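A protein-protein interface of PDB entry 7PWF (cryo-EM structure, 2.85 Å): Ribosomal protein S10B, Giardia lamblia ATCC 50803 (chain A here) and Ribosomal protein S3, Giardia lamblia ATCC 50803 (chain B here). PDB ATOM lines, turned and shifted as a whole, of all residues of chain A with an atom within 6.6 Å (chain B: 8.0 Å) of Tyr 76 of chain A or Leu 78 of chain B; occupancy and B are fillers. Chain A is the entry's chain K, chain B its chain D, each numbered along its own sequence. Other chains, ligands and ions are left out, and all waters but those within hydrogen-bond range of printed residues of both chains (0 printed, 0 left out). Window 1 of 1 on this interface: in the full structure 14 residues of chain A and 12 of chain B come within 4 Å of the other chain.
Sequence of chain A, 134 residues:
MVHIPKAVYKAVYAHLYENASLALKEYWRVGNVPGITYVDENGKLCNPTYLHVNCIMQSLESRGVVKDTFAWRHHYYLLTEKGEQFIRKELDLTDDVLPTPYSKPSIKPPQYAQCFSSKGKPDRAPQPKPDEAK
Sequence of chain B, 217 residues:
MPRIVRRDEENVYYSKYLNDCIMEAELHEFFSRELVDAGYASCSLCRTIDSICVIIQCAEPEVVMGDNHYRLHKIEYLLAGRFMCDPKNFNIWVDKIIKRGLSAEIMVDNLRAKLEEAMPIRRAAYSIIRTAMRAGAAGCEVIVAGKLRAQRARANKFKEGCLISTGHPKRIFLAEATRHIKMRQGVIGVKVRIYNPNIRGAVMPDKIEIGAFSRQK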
ATOM      1  N   ASN A  19      -9.677 -15.223  -9.960  1.00  0.00           N
ATOM      2  CA  ASN A  19     -10.500 -14.051 -10.218  1.00  0.00           C
ATOM      3  C   ASN A  19     -10.882 -13.252  -8.972  1.00  0.00           C
ATOM      4  O   ASN A  19     -11.556 -12.225  -9.112  1.00  0.00           O
ATOM      5  CB  ASN A  19     -11.782 -14.464 -10.949  1.00  0.00           C
ATOM      6  CG  ASN A  19     -11.525 -15.425 -12.093  1.00  0.00           C
ATOM      7  OD1 ASN A  19     -11.990 -16.562 -12.067  1.00  0.00           O
ATOM      8  ND2 ASN A  19     -10.770 -14.983 -13.090  1.00  0.00           N
ATOM      9  N   ALA A  20     -10.484 -13.679  -7.772  1.00  0.00           N
ATOM     10  CA  ALA A  20     -10.879 -12.962  -6.561  1.00  0.00           C
ATOM     11  C   ALA A  20     -10.373 -11.523  -6.585  1.00  0.00           C
ATOM     12  O   ALA A  20      -9.272 -11.244  -7.067  1.00  0.00           O
ATOM     13  CB  ALA A  20     -10.357 -13.678  -5.314  1.00  0.00           C
ATOM     14  N   SER A  21     -11.200 -10.609  -6.065  1.00  0.00           N
ATOM     15  CA  SER A  21     -10.923  -9.177  -6.063  1.00  0.00           C
ATOM     16  C   SER A  21     -11.346  -8.569  -4.727  1.00  0.00           C
ATOM     17  O   SER A  21     -12.096  -9.171  -3.955  1.00  0.00           O
ATOM     18  CB  SER A  21     -11.628  -8.460  -7.219  1.00  0.00           C
ATOM     19  OG  SER A  21     -10.985  -8.732  -8.452  1.00  0.00           O
ATOM     20  N   LEU A  22     -10.869  -7.352  -4.474  1.00  0.00           N
ATOM     21  CA  LEU A  22     -10.879  -6.763  -3.140  1.00  0.00           C
ATOM     22  C   LEU A  22     -11.790  -5.541  -3.060  1.00  0.00           C
ATOM     23  O   LEU A  22     -11.766  -4.679  -3.945  1.00  0.00           O
ATOM     24  CB  LEU A  22      -9.456  -6.391  -2.731  1.00  0.00           C
ATOM     25  CG  LEU A  22      -9.205  -5.783  -1.355  1.00  0.00           C
ATOM     26  CD1 LEU A  22     -10.000  -6.498  -0.288  1.00  0.00           C
ATOM     27  CD2 LEU A  22      -7.737  -5.916  -1.066  1.00  0.00           C
ATOM     28  N   ALA A  23     -12.582  -5.475  -1.988  1.00  0.00           N
ATOM     29  CA  ALA A  23     -13.374  -4.307  -1.622  1.00  0.00           C
ATOM     30  C   ALA A  23     -12.983  -3.857  -0.219  1.00  0.00           C
ATOM     31  O   ALA A  23     -12.661  -4.687   0.638  1.00  0.00           O
ATOM     32  CB  ALA A  23     -14.876  -4.612  -1.677  1.00  0.00           C
ATOM     33  N   LEU A  24     -13.015  -2.545   0.018  1.00  0.00           N
ATOM     34  CA  LEU A  24     -12.495  -1.962   1.248  1.00  0.00           C
ATOM     35  C   LEU A  24     -13.434  -0.878   1.757  1.00  0.00           C
ATOM     36  O   LEU A  24     -13.913  -0.051   0.979  1.00  0.00           O
ATOM     37  CB  LEU A  24     -11.101  -1.374   1.019  1.00  0.00           C
ATOM     38  CG  LEU A  24     -10.284  -0.958   2.240  1.00  0.00           C
ATOM     39  CD1 LEU A  24      -9.975  -2.158   3.120  1.00  0.00           C
ATOM     40  CD2 LEU A  24      -9.008  -0.285   1.781  1.00  0.00           C
ATOM     41  N   LYS A  67      -7.018  -0.820 -10.706  1.00  0.00           N
ATOM     42  CA  LYS A  67      -7.916   0.268 -11.062  1.00  0.00           C
ATOM     43  C   LYS A  67      -9.057   0.319 -10.056  1.00  0.00           C
ATOM     44  O   LYS A  67      -9.557  -0.716  -9.612  1.00  0.00           O
ATOM     45  CB  LYS A  67      -8.471   0.100 -12.480  1.00  0.00           C
ATOM     46  CG  LYS A  67      -9.151  -1.239 -12.739  1.00  0.00           C
ATOM     47  CD  LYS A  67     -10.374  -1.071 -13.630  1.00  0.00           C
ATOM     48  CE  LYS A  67     -11.206  -2.343 -13.670  1.00  0.00           C
ATOM     49  NZ  LYS A  67     -12.497  -2.177 -14.387  1.00  0.00           N
ATOM     50  N   ASP A  68      -9.478   1.528  -9.694  1.00  0.00           N
ATOM     51  CA  ASP A  68     -10.502   1.656  -8.668  1.00  0.00           C
ATOM     52  C   ASP A  68     -11.636   2.562  -9.121  1.00  0.00           C
ATOM     53  O   ASP A  68     -11.447   3.493  -9.907  1.00  0.00           O
ATOM     54  CB  ASP A  68      -9.921   2.155  -7.323  1.00  0.00           C
ATOM     55  CG  ASP A  68      -9.745   3.670  -7.248  1.00  0.00           C
ATOM     56  OD1 ASP A  68      -9.646   4.353  -8.285  1.00  0.00           O
ATOM     57  OD2 ASP A  68      -9.713   4.189  -6.116  1.00  0.00           O
ATOM     58  N   THR A  69     -12.829   2.216  -8.667  1.00  0.00           N
ATOM     59  CA  THR A  69     -13.959   3.121  -8.575  1.00  0.00           C
ATOM     60  C   THR A  69     -14.318   3.254  -7.103  1.00  0.00           C
ATOM     61  O   THR A  69     -13.597   2.763  -6.226  1.00  0.00           O
ATOM     62  CB  THR A  69     -15.128   2.631  -9.432  1.00  0.00           C
ATOM     63  OG1 THR A  69     -15.860   1.618  -8.729  1.00  0.00           O
ATOM     64  CG2 THR A  69     -14.620   2.080 -10.746  1.00  0.00           C
ATOM     65  N   PHE A  70     -15.424   3.931  -6.815  1.00  0.00           N
ATOM     66  CA  PHE A  70     -15.796   4.107  -5.421  1.00  0.00           C
ATOM     67  C   PHE A  70     -17.288   4.395  -5.327  1.00  0.00           C
ATOM     68  O   PHE A  70     -17.836   5.117  -6.161  1.00  0.00           O
ATOM     69  CB  PHE A  70     -14.975   5.236  -4.788  1.00  0.00           C
ATOM     70  CG  PHE A  70     -15.232   5.426  -3.328  1.00  0.00           C
ATOM     71  CD1 PHE A  70     -14.477   4.741  -2.390  1.00  0.00           C
ATOM     72  CD2 PHE A  70     -16.214   6.297  -2.888  1.00  0.00           C
ATOM     73  CE1 PHE A  70     -14.707   4.908  -1.038  1.00  0.00           C
ATOM     74  CE2 PHE A  70     -16.443   6.468  -1.543  1.00  0.00           C
ATOM     75  CZ  PHE A  70     -15.684   5.775  -0.618  1.00  0.00           C
ATOM     76  N   ALA A  71     -17.930   3.847  -4.294  1.00  0.00           N
ATOM     77  CA  ALA A  71     -19.369   3.991  -4.114  1.00  0.00           C
ATOM     78  C   ALA A  71     -19.744   3.648  -2.678  1.00  0.00           C
ATOM     79  O   ALA A  71     -19.294   2.625  -2.153  1.00  0.00           O
ATOM     80  CB  ALA A  71     -20.127   3.084  -5.087  1.00  0.00           C
ATOM     81  N   TRP A  72     -20.578   4.489  -2.060  1.00  0.00           N
ATOM     82  CA  TRP A  72     -21.114   4.260  -0.714  1.00  0.00           C
ATOM     83  C   TRP A  72     -20.017   3.877   0.280  1.00  0.00           C
ATOM     84  O   TRP A  72     -20.000   2.776   0.836  1.00  0.00           O
ATOM     85  CB  TRP A  72     -22.212   3.193  -0.717  1.00  0.00           C
ATOM     86  CG  TRP A  72     -23.419   3.477  -1.557  1.00  0.00           C
ATOM     87  CD1 TRP A  72     -23.481   4.247  -2.671  1.00  0.00           C
ATOM     88  CD2 TRP A  72     -24.731   2.938  -1.370  1.00  0.00           C
ATOM     89  NE1 TRP A  72     -24.753   4.250  -3.176  1.00  0.00           N
ATOM     90  CE2 TRP A  72     -25.541   3.449  -2.397  1.00  0.00           C
ATOM     91  CE3 TRP A  72     -25.304   2.082  -0.422  1.00  0.00           C
ATOM     92  CZ2 TRP A  72     -26.889   3.136  -2.512  1.00  0.00           C
ATOM     93  CZ3 TRP A  72     -26.642   1.772  -0.534  1.00  0.00           C
ATOM     94  CH2 TRP A  72     -27.421   2.298  -1.574  1.00  0.00           C
ATOM     95  N   HIS A  74     -17.016   2.956   0.247  1.00  0.00           N
ATOM     96  CA  HIS A  74     -16.453   1.620   0.102  1.00  0.00           C
ATOM     97  C   HIS A  74     -15.598   1.567  -1.158  1.00  0.00           C
ATOM     98  O   HIS A  74     -16.093   1.834  -2.258  1.00  0.00           O
ATOM     99  CB  HIS A  74     -17.581   0.592   0.051  1.00  0.00           C
ATOM    100  CG  HIS A  74     -17.234  -0.721   0.671  1.00  0.00           C
ATOM    101  ND1 HIS A  74     -16.238  -1.538   0.185  1.00  0.00           N
ATOM    102  CD2 HIS A  74     -17.752  -1.354   1.748  1.00  0.00           C
ATOM    103  CE1 HIS A  74     -16.157  -2.620   0.938  1.00  0.00           C
ATOM    104  NE2 HIS A  74     -17.064  -2.533   1.893  1.00  0.00           N
ATOM    105  N   HIS A  75     -14.328   1.201  -0.995  1.00  0.00           N
ATOM    106  CA  HIS A  75     -13.322   1.291  -2.050  1.00  0.00           C
ATOM    107  C   HIS A  75     -13.365   0.032  -2.904  1.00  0.00           C
ATOM    108  O   HIS A  75     -13.011  -1.050  -2.433  1.00  0.00           O
ATOM    109  CB  HIS A  75     -11.935   1.465  -1.442  1.00  0.00           C
ATOM    110  CG  HIS A  75     -11.558   2.884  -1.178  1.00  0.00           C
ATOM    111  ND1 HIS A  75     -11.710   3.476   0.055  1.00  0.00           N
ATOM    112  CD2 HIS A  75     -11.035   3.831  -1.989  1.00  0.00           C
ATOM    113  CE1 HIS A  75     -11.297   4.729  -0.006  1.00  0.00           C
ATOM    114  NE2 HIS A  75     -10.882   4.970  -1.236  1.00  0.00           N
ATOM    115  N   TYR A  76     -13.784   0.168  -4.160  1.00  0.00           N
ATOM    116  CA  TYR A  76     -13.808  -0.962  -5.080  1.00  0.00           C
ATOM    117  C   TYR A  76     -12.576  -0.943  -5.977  1.00  0.00           C
ATOM    118  O   TYR A  76     -12.355   0.017  -6.726  1.00  0.00           O
ATOM    119  CB  TYR A  76     -15.074  -0.948  -5.935  1.00  0.00           C
ATOM    120  CG  TYR A  76     -16.362  -1.176  -5.179  1.00  0.00           C
ATOM    121  CD1 TYR A  76     -17.078  -0.106  -4.653  1.00  0.00           C
ATOM    122  CD2 TYR A  76     -16.876  -2.456  -5.009  1.00  0.00           C
ATOM    123  CE1 TYR A  76     -18.261  -0.304  -3.971  1.00  0.00           C
ATOM    124  CE2 TYR A  76     -18.062  -2.664  -4.332  1.00  0.00           C
ATOM    125  CZ  TYR A  76     -18.749  -1.587  -3.815  1.00  0.00           C
ATOM    126  OH  TYR A  76     -19.926  -1.790  -3.139  1.00  0.00           O
ATOM    127  N   TYR A  77     -11.798  -2.026  -5.912  1.00  0.00           N
ATOM    128  CA  TYR A  77     -10.575  -2.222  -6.679  1.00  0.00           C
ATOM    129  C   TYR A  77     -10.720  -3.438  -7.584  1.00  0.00           C
ATOM    130  O   TYR A  77     -11.399  -4.408  -7.235  1.00  0.00           O
ATOM    131  CB  TYR A  77      -9.360  -2.450  -5.763  1.00  0.00           C
ATOM    132  CG  TYR A  77      -8.938  -1.276  -4.906  1.00  0.00           C
ATOM    133  CD1 TYR A  77      -8.369  -0.150  -5.476  1.00  0.00           C
ATOM    134  CD2 TYR A  77      -9.060  -1.316  -3.525  1.00  0.00           C
ATOM    135  CE1 TYR A  77      -7.968   0.921  -4.703  1.00  0.00           C
ATOM    136  CE2 TYR A  77      -8.662  -0.244  -2.738  1.00  0.00           C
ATOM    137  CZ  TYR A  77      -8.115   0.869  -3.335  1.00  0.00           C
ATOM    138  OH  TYR A  77      -7.712   1.937  -2.566  1.00  0.00           O
ATOM    139  N   LEU A  78     -10.052  -3.391  -8.733  1.00  0.00           N
ATOM    140  CA  LEU A  78      -9.888  -4.544  -9.610  1.00  0.00           C
ATOM    141  C   LEU A  78      -8.425  -4.655 -10.011  1.00  0.00           C
ATOM    142  O   LEU A  78      -7.798  -3.657 -10.386  1.00  0.00           O
ATOM    143  CB  LEU A  78     -10.772  -4.448 -10.865  1.00  0.00           C
ATOM    144  CG  LEU A  78     -12.298  -4.567 -10.753  1.00  0.00           C
ATOM    145  CD1 LEU A  78     -12.916  -4.997 -12.069  1.00  0.00           C
ATOM    146  CD2 LEU A  78     -12.648  -5.599  -9.709  1.00  0.00           C
ATOM    147  N   MET B  23     -29.442  -3.434  -0.776  1.00  0.00           N
ATOM    148  CA  MET B  23     -28.309  -3.986  -1.509  1.00  0.00           C
ATOM    149  C   MET B  23     -28.505  -3.868  -3.017  1.00  0.00           C
ATOM    150  O   MET B  23     -27.534  -3.669  -3.754  1.00  0.00           O
ATOM    151  CB  MET B  23     -28.105  -5.443  -1.092  1.00  0.00           C
ATOM    152  CG  MET B  23     -27.096  -6.228  -1.907  1.00  0.00           C
ATOM    153  SD  MET B  23     -27.258  -8.006  -1.625  1.00  0.00           S
ATOM    154  CE  MET B  23     -26.508  -8.659  -3.108  1.00  0.00           C
ATOM    155  N   GLU B  26     -27.325  -0.412  -3.830  1.00  0.00           N
ATOM    156  CA  GLU B  26     -25.861  -0.450  -3.836  1.00  0.00           C
ATOM    157  C   GLU B  26     -25.324  -0.979  -5.168  1.00  0.00           C
ATOM    158  O   GLU B  26     -24.457  -0.358  -5.804  1.00  0.00           O
ATOM    159  CB  GLU B  26     -25.368  -1.320  -2.678  1.00  0.00           C
ATOM    160  CG  GLU B  26     -23.854  -1.433  -2.554  1.00  0.00           C
ATOM    161  CD  GLU B  26     -23.213  -0.316  -1.762  1.00  0.00           C
ATOM    162  OE1 GLU B  26     -22.510   0.510  -2.373  1.00  0.00           O
ATOM    163  OE2 GLU B  26     -23.384  -0.287  -0.527  1.00  0.00           O
ATOM    164  N   LEU B  27     -25.845  -2.128  -5.608  1.00  0.00           N
ATOM    165  CA  LEU B  27     -25.348  -2.762  -6.826  1.00  0.00           C
ATOM    166  C   LEU B  27     -25.631  -1.910  -8.057  1.00  0.00           C
ATOM    167  O   LEU B  27     -24.773  -1.783  -8.940  1.00  0.00           O
ATOM    168  CB  LEU B  27     -25.966  -4.150  -6.989  1.00  0.00           C
ATOM    169  CG  LEU B  27     -25.743  -5.174  -5.876  1.00  0.00           C
ATOM    170  CD1 LEU B  27     -26.736  -6.304  -5.999  1.00  0.00           C
ATOM    171  CD2 LEU B  27     -24.318  -5.709  -5.875  1.00  0.00           C
ATOM    172  N   GLU B  29     -25.925   1.347  -8.193  1.00  0.00           N
ATOM    173  CA  GLU B  29     -25.055   2.517  -8.187  1.00  0.00           C
ATOM    174  C   GLU B  29     -23.639   2.151  -8.625  1.00  0.00           C
ATOM    175  O   GLU B  29     -23.005   2.887  -9.399  1.00  0.00           O
ATOM    176  CB  GLU B  29     -25.057   3.138  -6.789  1.00  0.00           C
ATOM    177  CG  GLU B  29     -24.880   4.640  -6.747  1.00  0.00           C
ATOM    178  CD  GLU B  29     -23.439   5.058  -6.790  1.00  0.00           C
ATOM    179  OE1 GLU B  29     -23.169   6.264  -6.956  1.00  0.00           O
ATOM    180  OE2 GLU B  29     -22.572   4.176  -6.671  1.00  0.00           O
ATOM    181  N   PHE B  30     -23.129   1.015  -8.138  1.00  0.00           N
ATOM    182  CA  PHE B  30     -21.795   0.586  -8.543  1.00  0.00           C
ATOM    183  C   PHE B  30     -21.741   0.261 -10.034  1.00  0.00           C
ATOM    184  O   PHE B  30     -20.776   0.622 -10.716  1.00  0.00           O
ATOM    185  CB  PHE B  30     -21.350  -0.619  -7.719  1.00  0.00           C
ATOM    186  CG  PHE B  30     -20.186  -1.354  -8.316  1.00  0.00           C
ATOM    187  CD1 PHE B  30     -18.928  -0.784  -8.322  1.00  0.00           C
ATOM    188  CD2 PHE B  30     -20.352  -2.602  -8.891  1.00  0.00           C
ATOM    189  CE1 PHE B  30     -17.856  -1.448  -8.877  1.00  0.00           C
ATOM    190  CE2 PHE B  30     -19.284  -3.266  -9.446  1.00  0.00           C
ATOM    191  CZ  PHE B  30     -18.033  -2.684  -9.437  1.00  0.00           C
ATOM    192  N   PHE B  31     -22.763  -0.423 -10.560  1.00  0.00           N
ATOM    193  CA  PHE B  31     -22.784  -0.694 -11.995  1.00  0.00           C
ATOM    194  C   PHE B  31     -22.799   0.595 -12.797  1.00  0.00           C
ATOM    195  O   PHE B  31     -22.069   0.717 -13.782  1.00  0.00           O
ATOM    196  CB  PHE B  31     -23.971  -1.577 -12.375  1.00  0.00           C
ATOM    197  CG  PHE B  31     -23.891  -2.970 -11.834  1.00  0.00           C
ATOM    198  CD1 PHE B  31     -22.681  -3.501 -11.427  1.00  0.00           C
ATOM    199  CD2 PHE B  31     -25.020  -3.757 -11.748  1.00  0.00           C
ATOM    200  CE1 PHE B  31     -22.603  -4.780 -10.935  1.00  0.00           C
ATOM    201  CE2 PHE B  31     -24.943  -5.041 -11.253  1.00  0.00           C
ATOM    202  CZ  PHE B  31     -23.736  -5.548 -10.846  1.00  0.00           C
ATOM    203  N   GLU B  34     -19.225   2.277 -12.578  1.00  0.00           N
ATOM    204  CA  GLU B  34     -18.116   1.513 -13.136  1.00  0.00           C
ATOM    205  C   GLU B  34     -18.347   1.146 -14.597  1.00  0.00           C
ATOM    206  O   GLU B  34     -17.497   1.433 -15.444  1.00  0.00           O
ATOM    207  CB  GLU B  34     -17.862   0.254 -12.288  1.00  0.00           C
ATOM    208  CG  GLU B  34     -16.455  -0.365 -12.410  1.00  0.00           C
ATOM    209  CD  GLU B  34     -16.101  -0.928 -13.788  1.00  0.00           C
ATOM    210  OE1 GLU B  34     -17.013  -1.223 -14.582  1.00  0.00           O
ATOM    211  OE2 GLU B  34     -14.893  -1.059 -14.079  1.00  0.00           O
ATOM    212  N   LEU B  72     -15.854 -10.348 -16.629  1.00  0.00           N
ATOM    213  CA  LEU B  72     -17.142 -10.626 -16.000  1.00  0.00           C
ATOM    214  C   LEU B  72     -16.962 -11.324 -14.660  1.00  0.00           C
ATOM    215  O   LEU B  72     -17.495 -10.873 -13.639  1.00  0.00           O
ATOM    216  CB  LEU B  72     -18.013 -11.470 -16.929  1.00  0.00           C
ATOM    217  CG  LEU B  72     -19.410 -11.805 -16.395  1.00  0.00           C
ATOM    218  CD1 LEU B  72     -20.374 -10.661 -16.660  1.00  0.00           C
ATOM    219  CD2 LEU B  72     -19.943 -13.108 -16.979  1.00  0.00           C
ATOM    220  N   HIS B  73     -16.185 -12.413 -14.636  1.00  0.00           N
ATOM    221  CA  HIS B  73     -16.033 -13.187 -13.406  1.00  0.00           C
ATOM    222  C   HIS B  73     -15.313 -12.389 -12.331  1.00  0.00           C
ATOM    223  O   HIS B  73     -15.652 -12.493 -11.147  1.00  0.00           O
ATOM    224  CB  HIS B  73     -15.299 -14.499 -13.682  1.00  0.00           C
ATOM    225  CG  HIS B  73     -16.080 -15.461 -14.520  1.00  0.00           C
ATOM    226  ND1 HIS B  73     -15.663 -15.872 -15.767  1.00  0.00           N
ATOM    227  CD2 HIS B  73     -17.267 -16.074 -14.300  1.00  0.00           C
ATOM    228  CE1 HIS B  73     -16.549 -16.713 -16.269  1.00  0.00           C
ATOM    229  NE2 HIS B  73     -17.533 -16.851 -15.401  1.00  0.00           N
ATOM    230  N   LYS B  74     -14.322 -11.585 -12.716  1.00  0.00           N
ATOM    231  CA  LYS B  74     -13.670 -10.713 -11.746  1.00  0.00           C
ATOM    232  C   LYS B  74     -14.653  -9.754 -11.087  1.00  0.00           C
ATOM    233  O   LYS B  74     -14.391  -9.286  -9.974  1.00  0.00           O
ATOM    234  CB  LYS B  74     -12.541  -9.933 -12.419  1.00  0.00           C
ATOM    235  N   ILE B  75     -15.771  -9.441 -11.749  1.00  0.00           N
ATOM    236  CA  ILE B  75     -16.846  -8.708 -11.085  1.00  0.00           C
ATOM    237  C   ILE B  75     -17.543  -9.590 -10.058  1.00  0.00           C
ATOM    238  O   ILE B  75     -17.919  -9.126  -8.975  1.00  0.00           O
ATOM    239  CB  ILE B  75     -17.836  -8.143 -12.119  1.00  0.00           C
ATOM    240  CG1 ILE B  75     -17.104  -7.334 -13.191  1.00  0.00           C
ATOM    241  CG2 ILE B  75     -18.920  -7.331 -11.451  1.00  0.00           C
ATOM    242  CD1 ILE B  75     -16.649  -5.960 -12.738  1.00  0.00           C
ATOM    243  N   GLU B  76     -17.723 -10.874 -10.371  1.00  0.00           N
ATOM    244  CA  GLU B  76     -18.440 -11.790  -9.491  1.00  0.00           C
ATOM    245  C   GLU B  76     -17.715 -12.066  -8.180  1.00  0.00           C
ATOM    246  O   GLU B  76     -18.255 -12.800  -7.346  1.00  0.00           O
ATOM    247  CB  GLU B  76     -18.696 -13.110 -10.212  1.00  0.00           C
ATOM    248  CG  GLU B  76     -19.850 -13.072 -11.181  1.00  0.00           C
ATOM    249  CD  GLU B  76     -20.604 -14.375 -11.202  1.00  0.00           C
ATOM    250  OE1 GLU B  76     -21.174 -14.725 -12.256  1.00  0.00           O
ATOM    251  OE2 GLU B  76     -20.614 -15.056 -10.157  1.00  0.00           O
ATOM    252  N   TYR B  77     -16.516 -11.521  -7.979  1.00  0.00           N
ATOM    253  CA  TYR B  77     -15.807 -11.639  -6.714  1.00  0.00           C
ATOM    254  C   TYR B  77     -15.814 -10.358  -5.906  1.00  0.00           C
ATOM    255  O   TYR B  77     -15.441 -10.389  -4.728  1.00  0.00           O
ATOM    256  CB  TYR B  77     -14.361 -12.089  -6.950  1.00  0.00           C
ATOM    257  CG  TYR B  77     -14.246 -13.562  -7.260  1.00  0.00           C
ATOM    258  CD1 TYR B  77     -14.077 -14.491  -6.243  1.00  0.00           C
ATOM    259  CD2 TYR B  77     -14.344 -14.030  -8.564  1.00  0.00           C
ATOM    260  CE1 TYR B  77     -13.977 -15.842  -6.515  1.00  0.00           C
ATOM    261  CE2 TYR B  77     -14.252 -15.381  -8.843  1.00  0.00           C
ATOM    262  CZ  TYR B  77     -14.068 -16.283  -7.817  1.00  0.00           C
ATOM    263  OH  TYR B  77     -13.974 -17.627  -8.094  1.00  0.00           O
ATOM    264  N   LEU B  78     -16.216  -9.238  -6.502  1.00  0.00           N
ATOM    265  CA  LEU B  78     -16.522  -8.044  -5.735  1.00  0.00           C
ATOM    266  C   LEU B  78     -17.892  -8.118  -5.075  1.00  0.00           C
ATOM    267  O   LEU B  78     -18.169  -7.323  -4.171  1.00  0.00           O
ATOM    268  CB  LEU B  78     -16.443  -6.807  -6.634  1.00  0.00           C
ATOM    269  CG  LEU B  78     -15.139  -6.011  -6.553  1.00  0.00           C
ATOM    270  CD1 LEU B  78     -15.215  -4.775  -7.428  1.00  0.00           C
ATOM    271  CD2 LEU B  78     -14.821  -5.637  -5.117  1.00  0.00           C
ATOM    272  N   LEU B  79     -18.748  -9.051  -5.496  1.00  0.00           N
ATOM    273  CA  LEU B  79     -20.034  -9.252  -4.841  1.00  0.00           C
ATOM    274  C   LEU B  79     -19.921 -10.058  -3.555  1.00  0.00           C
ATOM    275  O   LEU B  79     -20.806  -9.957  -2.700  1.00  0.00           O
ATOM    276  CB  LEU B  79     -21.017  -9.947  -5.784  1.00  0.00           C
ATOM    277  CG  LEU B  79     -22.036  -9.083  -6.528  1.00  0.00           C
ATOM    278  CD1 LEU B  79     -21.364  -7.948  -7.282  1.00  0.00           C
ATOM    279  CD2 LEU B  79     -22.882  -9.954  -7.459  1.00  0.00           C
ATOM    280  N   ALA B  80     -18.863 -10.856  -3.398  1.00  0.00           N
ATOM    281  CA  ALA B  80     -18.699 -11.628  -2.173  1.00  0.00           C
ATOM    282  C   ALA B  80     -18.108 -10.791  -1.046  1.00  0.00           C
ATOM    283  O   ALA B  80     -18.426 -11.024   0.126  1.00  0.00           O
ATOM    284  CB  ALA B  80     -17.828 -12.855  -2.435  1.00  0.00           C
ATOM    285  N   GLY B  81     -17.260  -9.822  -1.370  1.00  0.00           N
ATOM    286  CA  GLY B  81     -16.768  -8.893  -0.375  1.00  0.00           C
ATOM    287  C   GLY B  81     -17.879  -8.045   0.222  1.00  0.00           C
ATOM    288  O   GLY B  81     -18.743  -7.535  -0.491  1.00  0.00           O
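Of the printed residues of chain B, Thr 69 of chain A touches Phe 30 and Glu 34.
Of the printed residues of chain B, Tyr 76 of chain A touches Glu 26, Phe 30 and Leu 78.
Of the printed residues of chain B, Tyr 77 of chain A touches Leu 78.
Of the printed residues of chain A, Glu 26 of chain B touches Ala 71 (3.9 Å), Trp 72 (3.1 Å) and Tyr 76 (3.5 Å).
Of the printed residues of chain A, Lys 74 of chain B touches Asn 19 (3.7 Å) and Ser 21 (3.8 Å).
Leu 78 of chain B touches five residues of chain A.
The nearest residue of chain A that does not touch Leu 78 of chain B is Ser 21 of chain A (4.3 Å).
The nearest printed residue of chain A that does not touch Glu 26 of chain B is His 74 of chain A (5.5 Å).
The side-chain carboxylate (OE2) of Glu 34 of chain B lies within salt-bridge range of the side-chain amino group (NZ) of Lys 67 of chain A (2.7 Å).
O of Leu 22 of chain A lies within hydrogen-bond range of N of Tyr 77 of chain A (3.3 Å).
O of Lys 67 of chain A is in hydrogen-bond range of N of Leu 78 of chain A (2.9 Å).
The backbone NH (N) of Thr 69 of chain A sits at hydrogen-bond distance from the backbone carbonyl oxygen (O) of Tyr 76 of chain A (3.0 Å).
Among the printed residues, merely in contact across the chains: Trp 72 of chain A with Glu 26 of chain B (3.1 Å), Ala 71 of chain A with Glu 29 of chain B (3.1 Å), Asn 19 of chain A with Tyr 77 of chain B (3.4 Å), Leu 22 of chain A with Leu 78 of chain B (3.4 Å), Thr 69 of chain A with Glu 34 of chain B (3.5 Å), Ala 20 of chain A with Tyr 77 of chain B (3.5 Å), Leu 78 of chain A with Leu 78 of chain B (3.5 Å), Tyr 76 of chain A with Glu 26 of chain B (3.5 Å), Ala 23 of chain A with Leu 78 of chain B (3.6 Å), Trp 72 of chain A with Glu 29 of chain B (3.6 Å), Ser 21 of chain A with Tyr 77 of chain B (3.6 Å), Thr 69 of chain A with Phe 30 of chain B (3.7 Å), Asn 19 of chain A with Lys 74 of chain B (3.7 Å), Tyr 76 of chain A with Leu 78 of chain B (3.7 Å), Ser 21 of chain A with Lys 74 of chain B (3.8 Å), Tyr 77 of chain A with Leu 78 of chain B (3.8 Å), Ala 71 of chain A with Glu 26 of chain B (3.9 Å), Leu 78 of chain A with Ile 75 of chain B (3.9 Å) and Tyr 76 of chain A with Phe 30 of chain B (3.998 Å).
Of the 17 printed residues of chain B, 8 touch a printed residue of chain A.
Hydrophobic or aromatic side chains of chain B that line the printed part of chain A: Phe 30, Ile 75, Tyr 77 and Leu 78.
Along chain B the printed residues that touch a printed residue of chain A span positions 26 to 78.
Printed residues of chain A that touch a printed residue of chain B: Asn 19, Ala 20, Ser 21, Leu 22, Ala 23, Lys 67, Thr 69, Ala 71, Trp 72, Tyr 76, Tyr 77 and Leu 78.
Hydrophobic or aromatic side chains of chain A within 4 Å of the printed part of chain B: Ala 20, Ala 23, Ala 71, Trp 72, Tyr 76 and Leu 78.
Among the printed residues, Asp or Glu carboxylates within 4 Å of a Lys or Arg side-chain nitrogen of the other chain: Lys 67 of chain A with Glu 34 of chain B (2.7 Å).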
